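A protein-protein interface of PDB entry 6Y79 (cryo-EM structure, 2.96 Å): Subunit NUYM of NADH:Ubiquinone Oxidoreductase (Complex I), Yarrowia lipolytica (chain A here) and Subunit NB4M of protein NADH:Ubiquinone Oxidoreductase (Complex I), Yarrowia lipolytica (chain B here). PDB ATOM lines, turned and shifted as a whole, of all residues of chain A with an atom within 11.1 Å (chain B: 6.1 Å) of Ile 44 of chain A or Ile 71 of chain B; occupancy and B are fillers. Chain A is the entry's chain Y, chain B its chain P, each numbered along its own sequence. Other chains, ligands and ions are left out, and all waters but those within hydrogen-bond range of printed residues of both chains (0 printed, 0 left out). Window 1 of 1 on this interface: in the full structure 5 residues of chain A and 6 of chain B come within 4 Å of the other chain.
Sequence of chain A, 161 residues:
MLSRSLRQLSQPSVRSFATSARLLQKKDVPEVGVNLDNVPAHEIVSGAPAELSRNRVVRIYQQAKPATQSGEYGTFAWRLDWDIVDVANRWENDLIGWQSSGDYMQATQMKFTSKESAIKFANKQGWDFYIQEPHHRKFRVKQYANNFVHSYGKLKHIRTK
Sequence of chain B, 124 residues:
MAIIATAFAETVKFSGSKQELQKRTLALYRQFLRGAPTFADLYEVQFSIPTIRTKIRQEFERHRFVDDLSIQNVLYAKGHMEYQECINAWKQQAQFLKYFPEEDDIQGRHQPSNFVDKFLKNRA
Of the printed residues of chain B, Pro 40 of chain A touches Asp 68.
Of chain B, only Ile 71 (3.7 Å) comes within 4 Å of Ile 44 of chain A.
Of the printed residues of chain B, Val 45 of chain A touches Ile 71 (3.8 Å) and Val 74 (3.5 Å).
Arg 54 of chain A touches none of the printed residues of chain B.
No residue of chain A comes within 4 Å of Ser 70 of chain B.
Printed residues of chain A within 4 Å of Ile 71 of chain B: Ala 41 (3.4 Å), Ile 44 (3.7 Å) and Val 45 (3.8 Å).
No residue of chain A comes within 4 Å of Gln 72 of chain B.
No residue of chain A comes within 4 Å of Asn 73 of chain B.
No residue of chain A comes within 4 Å of Leu 75 of chain B.
The nearest printed residue of chain B that does not touch Val 45 of chain A is Leu 75 of chain B (5.1 Å).
Among the printed residues, merely in contact across the chains: Pro 40 of chain A with Asp 68 of chain B, Ala 41 of chain A with Ile 71 of chain B, Ile 44 of chain A with Ile 71 of chain B, Val 45 of chain A with Ile 71 of chain B and Val 45 of chain A with Val 74 of chain B.
O of Pro 40 of chain A sits at hydrogen-bond distance from ND1 of His 42 of chain A, at 3.3 Å.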
ATOM      1  N   VAL A  39       5.421 -21.676  32.214  1.00  0.00           N
ATOM      2  CA  VAL A  39       5.673 -21.515  30.786  1.00  0.00           C
ATOM      3  C   VAL A  39       6.641 -22.585  30.289  1.00  0.00           C
ATOM      4  O   VAL A  39       7.808 -22.602  30.680  1.00  0.00           O
ATOM      5  CB  VAL A  39       6.208 -20.111  30.468  1.00  0.00           C
ATOM      6  CG1 VAL A  39       6.571 -20.008  28.998  1.00  0.00           C
ATOM      7  CG2 VAL A  39       5.181 -19.055  30.852  1.00  0.00           C
ATOM      8  N   PRO A  40       6.149 -23.487  29.440  1.00  0.00           N
ATOM      9  CA  PRO A  40       7.014 -24.546  28.905  1.00  0.00           C
ATOM     10  C   PRO A  40       8.025 -23.998  27.905  1.00  0.00           C
ATOM     11  O   PRO A  40       7.727 -23.101  27.117  1.00  0.00           O
ATOM     12  CB  PRO A  40       6.024 -25.508  28.240  1.00  0.00           C
ATOM     13  CG  PRO A  40       4.823 -24.672  27.950  1.00  0.00           C
ATOM     14  CD  PRO A  40       4.740 -23.668  29.048  1.00  0.00           C
ATOM     15  N   ALA A  41       9.229 -24.559  27.943  1.00  0.00           N
ATOM     16  CA  ALA A  41      10.362 -24.038  27.186  1.00  0.00           C
ATOM     17  C   ALA A  41      10.558 -24.872  25.924  1.00  0.00           C
ATOM     18  O   ALA A  41      11.160 -25.948  25.970  1.00  0.00           O
ATOM     19  CB  ALA A  41      11.621 -24.040  28.050  1.00  0.00           C
ATOM     20  N   HIS A  42      10.072 -24.359  24.793  1.00  0.00           N
ATOM     21  CA  HIS A  42      10.051 -25.084  23.530  1.00  0.00           C
ATOM     22  C   HIS A  42      11.267 -24.812  22.658  1.00  0.00           C
ATOM     23  O   HIS A  42      11.336 -25.329  21.541  1.00  0.00           O
ATOM     24  CB  HIS A  42       8.794 -24.730  22.742  1.00  0.00           C
ATOM     25  CG  HIS A  42       7.533 -25.288  23.317  1.00  0.00           C
ATOM     26  ND1 HIS A  42       6.914 -24.738  24.416  1.00  0.00           N
ATOM     27  CD2 HIS A  42       6.751 -26.320  22.923  1.00  0.00           C
ATOM     28  CE1 HIS A  42       5.813 -25.416  24.684  1.00  0.00           C
ATOM     29  NE2 HIS A  42       5.691 -26.381  23.792  1.00  0.00           N
ATOM     30  N   GLU A  43      12.222 -24.012  23.132  1.00  0.00           N
ATOM     31  CA  GLU A  43      13.345 -23.618  22.295  1.00  0.00           C
ATOM     32  C   GLU A  43      14.352 -24.736  22.098  1.00  0.00           C
ATOM     33  O   GLU A  43      15.189 -24.645  21.194  1.00  0.00           O
ATOM     34  CB  GLU A  43      14.053 -22.404  22.888  1.00  0.00           C
ATOM     35  CG  GLU A  43      14.676 -22.647  24.244  1.00  0.00           C
ATOM     36  CD  GLU A  43      13.932 -21.952  25.361  1.00  0.00           C
ATOM     37  OE1 GLU A  43      12.730 -22.229  25.540  1.00  0.00           O
ATOM     38  OE2 GLU A  43      14.553 -21.127  26.064  1.00  0.00           O
ATOM     39  N   ILE A  44      14.295 -25.783  22.921  1.00  0.00           N
ATOM     40  CA  ILE A  44      15.203 -26.910  22.759  1.00  0.00           C
ATOM     41  C   ILE A  44      14.666 -27.943  21.782  1.00  0.00           C
ATOM     42  O   ILE A  44      15.434 -28.787  21.297  1.00  0.00           O
ATOM     43  CB  ILE A  44      15.503 -27.536  24.137  1.00  0.00           C
ATOM     44  CG1 ILE A  44      14.233 -28.068  24.779  1.00  0.00           C
ATOM     45  CG2 ILE A  44      16.084 -26.496  25.074  1.00  0.00           C
ATOM     46  CD1 ILE A  44      14.486 -28.888  25.992  1.00  0.00           C
ATOM     47  N   VAL A  45      13.372 -27.904  21.470  1.00  0.00           N
ATOM     48  CA  VAL A  45      12.731 -28.870  20.588  1.00  0.00           C
ATOM     49  C   VAL A  45      12.252 -28.253  19.288  1.00  0.00           C
ATOM     50  O   VAL A  45      11.622 -28.941  18.479  1.00  0.00           O
ATOM     51  CB  VAL A  45      11.572 -29.569  21.314  1.00  0.00           C
ATOM     52  CG1 VAL A  45      12.114 -30.037  22.617  1.00  0.00           C
ATOM     53  CG2 VAL A  45      10.431 -28.593  21.557  1.00  0.00           C
ATOM     54  N   SER A  46      12.543 -26.979  19.058  1.00  0.00           N
ATOM     55  CA  SER A  46      12.199 -26.319  17.812  1.00  0.00           C
ATOM     56  C   SER A  46      13.207 -26.582  16.709  1.00  0.00           C
ATOM     57  O   SER A  46      12.870 -26.430  15.530  1.00  0.00           O
ATOM     58  CB  SER A  46      12.097 -24.818  18.039  1.00  0.00           C
ATOM     59  OG  SER A  46      13.387 -24.251  18.080  1.00  0.00           O
ATOM     60  N   GLY A  47      14.430 -26.964  17.059  1.00  0.00           N
ATOM     61  CA  GLY A  47      15.494 -27.050  16.093  1.00  0.00           C
ATOM     62  C   GLY A  47      16.213 -25.751  15.831  1.00  0.00           C
ATOM     63  O   GLY A  47      17.201 -25.752  15.092  1.00  0.00           O
ATOM     64  N   ALA A  48      15.752 -24.645  16.401  1.00  0.00           N
ATOM     65  CA  ALA A  48      16.452 -23.386  16.249  1.00  0.00           C
ATOM     66  C   ALA A  48      17.729 -23.401  17.084  1.00  0.00           C
ATOM     67  O   ALA A  48      17.795 -24.075  18.116  1.00  0.00           O
ATOM     68  CB  ALA A  48      15.557 -22.224  16.670  1.00  0.00           C
ATOM     69  N   PRO A  49      18.768 -22.697  16.643  1.00  0.00           N
ATOM     70  CA  PRO A  49      20.023 -22.670  17.403  1.00  0.00           C
ATOM     71  C   PRO A  49      19.889 -21.889  18.701  1.00  0.00           C
ATOM     72  O   PRO A  49      18.941 -21.135  18.920  1.00  0.00           O
ATOM     73  CB  PRO A  49      20.999 -21.989  16.439  1.00  0.00           C
ATOM     74  CG  PRO A  49      20.130 -21.225  15.495  1.00  0.00           C
ATOM     75  CD  PRO A  49      18.928 -22.081  15.316  1.00  0.00           C
ATOM     76  N   ALA A  50      20.869 -22.099  19.581  1.00  0.00           N
ATOM     77  CA  ALA A  50      20.891 -21.370  20.841  1.00  0.00           C
ATOM     78  C   ALA A  50      21.210 -19.897  20.633  1.00  0.00           C
ATOM     79  O   ALA A  50      20.780 -19.063  21.442  1.00  0.00           O
ATOM     80  CB  ALA A  50      21.893 -22.010  21.799  1.00  0.00           C
ATOM     81  N   GLU A  51      21.945 -19.577  19.552  1.00  0.00           N
ATOM     82  CA  GLU A  51      22.353 -18.206  19.244  1.00  0.00           C
ATOM     83  C   GLU A  51      21.149 -17.277  19.091  1.00  0.00           C
ATOM     84  O   GLU A  51      21.201 -16.114  19.507  1.00  0.00           O
ATOM     85  CB  GLU A  51      23.230 -18.189  17.972  1.00  0.00           C
ATOM     86  CG  GLU A  51      22.507 -18.633  16.676  1.00  0.00           C
ATOM     87  CD  GLU A  51      23.348 -18.691  15.401  1.00  0.00           C
ATOM     88  OE1 GLU A  51      24.577 -18.472  15.422  1.00  0.00           O
ATOM     89  OE2 GLU A  51      22.749 -18.961  14.330  1.00  0.00           O
ATOM     90  N   LEU A  52      20.036 -17.799  18.577  1.00  0.00           N
ATOM     91  CA  LEU A  52      18.872 -16.980  18.273  1.00  0.00           C
ATOM     92  C   LEU A  52      18.103 -16.626  19.533  1.00  0.00           C
ATOM     93  O   LEU A  52      17.583 -15.514  19.666  1.00  0.00           O
ATOM     94  CB  LEU A  52      17.975 -17.730  17.285  1.00  0.00           C
ATOM     95  CG  LEU A  52      16.728 -17.050  16.743  1.00  0.00           C
ATOM     96  CD1 LEU A  52      17.118 -15.868  15.880  1.00  0.00           C
ATOM     97  CD2 LEU A  52      15.913 -18.058  15.967  1.00  0.00           C
ATOM     98  N   SER A  53      18.025 -17.561  20.466  1.00  0.00           N
ATOM     99  CA  SER A  53      17.329 -17.325  21.715  1.00  0.00           C
ATOM    100  C   SER A  53      18.188 -16.601  22.741  1.00  0.00           C
ATOM    101  O   SER A  53      17.636 -16.028  23.685  1.00  0.00           O
ATOM    102  CB  SER A  53      16.845 -18.649  22.296  1.00  0.00           C
ATOM    103  OG  SER A  53      16.592 -18.510  23.673  1.00  0.00           O
ATOM    104  N   ARG A  54      19.515 -16.599  22.598  1.00  0.00           N
ATOM    105  CA  ARG A  54      20.321 -15.934  23.609  1.00  0.00           C
ATOM    106  C   ARG A  54      20.945 -14.610  23.177  1.00  0.00           C
ATOM    107  O   ARG A  54      21.302 -13.817  24.052  1.00  0.00           O
ATOM    108  CB  ARG A  54      21.422 -16.874  24.123  1.00  0.00           C
ATOM    109  CG  ARG A  54      22.616 -17.026  23.211  1.00  0.00           C
ATOM    110  CD  ARG A  54      23.624 -18.018  23.764  1.00  0.00           C
ATOM    111  NE  ARG A  54      24.599 -18.411  22.752  1.00  0.00           N
ATOM    112  CZ  ARG A  54      25.642 -17.670  22.386  1.00  0.00           C
ATOM    113  NH1 ARG A  54      25.867 -16.491  22.953  1.00  0.00           N
ATOM    114  NH2 ARG A  54      26.473 -18.115  21.452  1.00  0.00           N
ATOM    115  N   ALA A 122       6.048 -15.662  22.171  1.00  0.00           N
ATOM    116  CA  ALA A 122       7.412 -15.154  22.206  1.00  0.00           C
ATOM    117  C   ALA A 122       8.173 -15.671  23.415  1.00  0.00           C
ATOM    118  O   ALA A 122       9.361 -15.998  23.307  1.00  0.00           O
ATOM    119  CB  ALA A 122       7.408 -13.628  22.191  1.00  0.00           C
ATOM    120  N   ASN A 123       7.525 -15.746  24.577  1.00  0.00           N
ATOM    121  CA  ASN A 123       8.224 -16.332  25.713  1.00  0.00           C
ATOM    122  C   ASN A 123       8.075 -17.847  25.771  1.00  0.00           C
ATOM    123  O   ASN A 123       8.791 -18.495  26.539  1.00  0.00           O
ATOM    124  CB  ASN A 123       7.796 -15.674  27.040  1.00  0.00           C
ATOM    125  CG  ASN A 123       6.307 -15.766  27.325  1.00  0.00           C
ATOM    126  OD1 ASN A 123       5.567 -16.527  26.711  1.00  0.00           O
ATOM    127  ND2 ASN A 123       5.861 -14.970  28.283  1.00  0.00           N
ATOM    128  N   LYS A 124       7.172 -18.419  24.976  1.00  0.00           N
ATOM    129  CA  LYS A 124       7.121 -19.866  24.822  1.00  0.00           C
ATOM    130  C   LYS A 124       8.296 -20.380  24.004  1.00  0.00           C
ATOM    131  O   LYS A 124       8.795 -21.482  24.249  1.00  0.00           O
ATOM    132  CB  LYS A 124       5.801 -20.260  24.172  1.00  0.00           C
ATOM    133  CG  LYS A 124       5.525 -21.728  24.157  1.00  0.00           C
ATOM    134  CD  LYS A 124       4.195 -22.015  23.508  1.00  0.00           C
ATOM    135  CE  LYS A 124       3.055 -21.520  24.365  1.00  0.00           C
ATOM    136  NZ  LYS A 124       1.745 -21.954  23.811  1.00  0.00           N
ATOM    137  N   GLN A 125       8.747 -19.605  23.024  1.00  0.00           N
ATOM    138  CA  GLN A 125       9.938 -19.946  22.260  1.00  0.00           C
ATOM    139  C   GLN A 125      11.216 -19.468  22.928  1.00  0.00           C
ATOM    140  O   GLN A 125      12.299 -19.704  22.389  1.00  0.00           O
ATOM    141  CB  GLN A 125       9.852 -19.359  20.851  1.00  0.00           C
ATOM    142  CG  GLN A 125       8.721 -19.896  19.999  1.00  0.00           C
ATOM    143  CD  GLN A 125       8.822 -21.378  19.758  1.00  0.00           C
ATOM    144  OE1 GLN A 125       7.927 -22.140  20.116  1.00  0.00           O
ATOM    145  NE2 GLN A 125       9.922 -21.803  19.157  1.00  0.00           N
ATOM    146  N   GLY A 126      11.118 -18.785  24.062  1.00  0.00           N
ATOM    147  CA  GLY A 126      12.291 -18.393  24.814  1.00  0.00           C
ATOM    148  C   GLY A 126      13.030 -17.192  24.278  1.00  0.00           C
ATOM    149  O   GLY A 126      14.264 -17.170  24.307  1.00  0.00           O
ATOM    150  N   TRP A 127      12.315 -16.182  23.798  1.00  0.00           N
ATOM    151  CA  TRP A 127      12.937 -15.039  23.147  1.00  0.00           C
ATOM    152  C   TRP A 127      12.850 -13.794  24.016  1.00  0.00           C
ATOM    153  O   TRP A 127      11.870 -13.576  24.732  1.00  0.00           O
ATOM    154  CB  TRP A 127      12.283 -14.749  21.796  1.00  0.00           C
ATOM    155  CG  TRP A 127      12.505 -15.815  20.788  1.00  0.00           C
ATOM    156  CD1 TRP A 127      13.456 -16.781  20.822  1.00  0.00           C
ATOM    157  CD2 TRP A 127      11.749 -16.036  19.600  1.00  0.00           C
ATOM    158  NE1 TRP A 127      13.347 -17.591  19.724  1.00  0.00           N
ATOM    159  CE2 TRP A 127      12.301 -17.154  18.959  1.00  0.00           C
ATOM    160  CE3 TRP A 127      10.656 -15.396  19.014  1.00  0.00           C
ATOM    161  CZ2 TRP A 127      11.804 -17.646  17.763  1.00  0.00           C
ATOM    162  CZ3 TRP A 127      10.163 -15.885  17.828  1.00  0.00           C
ATOM    163  CH2 TRP A 127      10.737 -16.997  17.213  1.00  0.00           C
ATOM    164  N   HIS B  63      20.864 -32.377  27.881  1.00  0.00           N
ATOM    165  CA  HIS B  63      19.429 -32.401  28.154  1.00  0.00           C
ATOM    166  C   HIS B  63      19.088 -33.123  29.453  1.00  0.00           C
ATOM    167  O   HIS B  63      18.131 -33.901  29.520  1.00  0.00           O
ATOM    168  CB  HIS B  63      18.675 -33.051  27.000  1.00  0.00           C
ATOM    169  CG  HIS B  63      18.624 -32.215  25.761  1.00  0.00           C
ATOM    170  ND1 HIS B  63      19.447 -32.441  24.681  1.00  0.00           N
ATOM    171  CD2 HIS B  63      17.853 -31.154  25.432  1.00  0.00           C
ATOM    172  CE1 HIS B  63      19.186 -31.553  23.740  1.00  0.00           C
ATOM    173  NE2 HIS B  63      18.223 -30.760  24.170  1.00  0.00           N
ATOM    174  N   VAL B  66      15.982 -31.134  32.099  1.00  0.00           N
ATOM    175  CA  VAL B  66      14.679 -30.815  31.529  1.00  0.00           C
ATOM    176  C   VAL B  66      13.608 -31.453  32.401  1.00  0.00           C
ATOM    177  O   VAL B  66      13.691 -32.639  32.737  1.00  0.00           O
ATOM    178  CB  VAL B  66      14.589 -31.306  30.076  1.00  0.00           C
ATOM    179  CG1 VAL B  66      13.332 -30.788  29.417  1.00  0.00           C
ATOM    180  CG2 VAL B  66      15.810 -30.858  29.306  1.00  0.00           C
ATOM    181  N   ASP B  68       9.827 -31.039  32.067  1.00  0.00           N
ATOM    182  CA  ASP B  68       8.498 -31.361  31.546  1.00  0.00           C
ATOM    183  C   ASP B  68       8.514 -32.661  30.753  1.00  0.00           C
ATOM    184  O   ASP B  68       9.361 -32.853  29.874  1.00  0.00           O
ATOM    185  CB  ASP B  68       7.969 -30.217  30.688  1.00  0.00           C
ATOM    186  CG  ASP B  68       7.870 -28.922  31.456  1.00  0.00           C
ATOM    187  OD1 ASP B  68       7.632 -28.977  32.684  1.00  0.00           O
ATOM    188  OD2 ASP B  68       8.015 -27.849  30.834  1.00  0.00           O
ATOM    189  N   LEU B  69       7.572 -33.546  31.083  1.00  0.00           N
ATOM    190  CA  LEU B  69       7.598 -34.924  30.610  1.00  0.00           C
ATOM    191  C   LEU B  69       7.343 -35.021  29.112  1.00  0.00           C
ATOM    192  O   LEU B  69       7.941 -35.862  28.433  1.00  0.00           O
ATOM    193  CB  LEU B  69       6.559 -35.734  31.383  1.00  0.00           C
ATOM    194  CG  LEU B  69       6.262 -37.164  30.945  1.00  0.00           C
ATOM    195  CD1 LEU B  69       7.422 -38.054  31.260  1.00  0.00           C
ATOM    196  CD2 LEU B  69       4.996 -37.686  31.589  1.00  0.00           C
ATOM    197  N   SER B  70       6.469 -34.158  28.583  1.00  0.00           N
ATOM    198  CA  SER B  70       6.189 -34.128  27.150  1.00  0.00           C
ATOM    199  C   SER B  70       7.393 -33.675  26.352  1.00  0.00           C
ATOM    200  O   SER B  70       7.677 -34.272  25.313  1.00  0.00           O
ATOM    201  CB  SER B  70       4.984 -33.236  26.847  1.00  0.00           C
ATOM    202  OG  SER B  70       5.016 -32.043  27.595  1.00  0.00           O
ATOM    203  N   ILE B  71       8.127 -32.662  26.839  1.00  0.00           N
ATOM    204  CA  ILE B  71       9.346 -32.228  26.163  1.00  0.00           C
ATOM    205  C   ILE B  71      10.424 -33.309  26.213  1.00  0.00           C
ATOM    206  O   ILE B  71      11.190 -33.501  25.251  1.00  0.00           O
ATOM    207  CB  ILE B  71       9.805 -30.903  26.787  1.00  0.00           C
ATOM    208  CG1 ILE B  71       8.774 -29.800  26.552  1.00  0.00           C
ATOM    209  CG2 ILE B  71      11.134 -30.435  26.239  1.00  0.00           C
ATOM    210  CD1 ILE B  71       9.176 -28.430  27.089  1.00  0.00           C
ATOM    211  N   GLN B  72      10.441 -34.103  27.276  1.00  0.00           N
ATOM    212  CA  GLN B  72      11.364 -35.226  27.293  1.00  0.00           C
ATOM    213  C   GLN B  72      10.904 -36.350  26.370  1.00  0.00           C
ATOM    214  O   GLN B  72      11.738 -37.086  25.833  1.00  0.00           O
ATOM    215  CB  GLN B  72      11.535 -35.734  28.713  1.00  0.00           C
ATOM    216  CG  GLN B  72      12.229 -34.815  29.666  1.00  0.00           C
ATOM    217  CD  GLN B  72      12.124 -35.334  31.077  1.00  0.00           C
ATOM    218  OE1 GLN B  72      11.407 -36.300  31.339  1.00  0.00           O
ATOM    219  NE2 GLN B  72      12.851 -34.714  31.992  1.00  0.00           N
ATOM    220  N   ASN B  73       9.595 -36.468  26.133  1.00  0.00           N
ATOM    221  CA  ASN B  73       9.102 -37.446  25.165  1.00  0.00           C
ATOM    222  C   ASN B  73       9.481 -37.056  23.747  1.00  0.00           C
ATOM    223  O   ASN B  73       9.889 -37.913  22.947  1.00  0.00           O
ATOM    224  CB  ASN B  73       7.586 -37.573  25.262  1.00  0.00           C
ATOM    225  CG  ASN B  73       7.143 -38.328  26.477  1.00  0.00           C
ATOM    226  OD1 ASN B  73       7.722 -39.348  26.824  1.00  0.00           O
ATOM    227  ND2 ASN B  73       6.102 -37.839  27.131  1.00  0.00           N
ATOM    228  N   VAL B  74       9.350 -35.765  23.418  1.00  0.00           N
ATOM    229  CA  VAL B  74       9.692 -35.313  22.072  1.00  0.00           C
ATOM    230  C   VAL B  74      11.202 -35.434  21.869  1.00  0.00           C
ATOM    231  O   VAL B  74      11.666 -35.817  20.789  1.00  0.00           O
ATOM    232  CB  VAL B  74       9.174 -33.876  21.794  1.00  0.00           C
ATOM    233  CG1 VAL B  74       7.801 -33.634  22.275  1.00  0.00           C
ATOM    234  CG2 VAL B  74      10.001 -32.836  22.315  1.00  0.00           C
ATOM    235  N   LEU B  75      11.972 -35.262  22.953  1.00  0.00           N
ATOM    236  CA  LEU B  75      13.418 -35.382  22.904  1.00  0.00           C
ATOM    237  C   LEU B  75      13.830 -36.827  22.695  1.00  0.00           C
ATOM    238  O   LEU B  75      14.746 -37.118  21.916  1.00  0.00           O
ATOM    239  CB  LEU B  75      13.963 -34.832  24.210  1.00  0.00           C
ATOM    240  CG  LEU B  75      15.384 -34.388  24.457  1.00  0.00           C
ATOM    241  CD1 LEU B  75      15.858 -33.481  23.360  1.00  0.00           C
ATOM    242  CD2 LEU B  75      15.307 -33.647  25.758  1.00  0.00           C
ATOM    243  N   TYR B  76      13.137 -37.751  23.364  1.00  0.00           N
ATOM    244  CA  TYR B  76      13.447 -39.167  23.218  1.00  0.00           C
ATOM    245  C   TYR B  76      13.103 -39.674  21.827  1.00  0.00           C
ATOM    246  O   TYR B  76      13.838 -40.498  21.263  1.00  0.00           O
ATOM    247  CB  TYR B  76      12.707 -39.982  24.277  1.00  0.00           C
ATOM    248  CG  TYR B  76      12.955 -41.460  24.129  1.00  0.00           C
ATOM    249  CD1 TYR B  76      14.193 -42.003  24.428  1.00  0.00           C
ATOM    250  CD2 TYR B  76      11.963 -42.309  23.659  1.00  0.00           C
ATOM    251  CE1 TYR B  76      14.429 -43.346  24.276  1.00  0.00           C
ATOM    252  CE2 TYR B  76      12.195 -43.651  23.501  1.00  0.00           C
ATOM    253  CZ  TYR B  76      13.426 -44.162  23.812  1.00  0.00           C
ATOM    254  OH  TYR B  76      13.654 -45.502  23.659  1.00  0.00           O
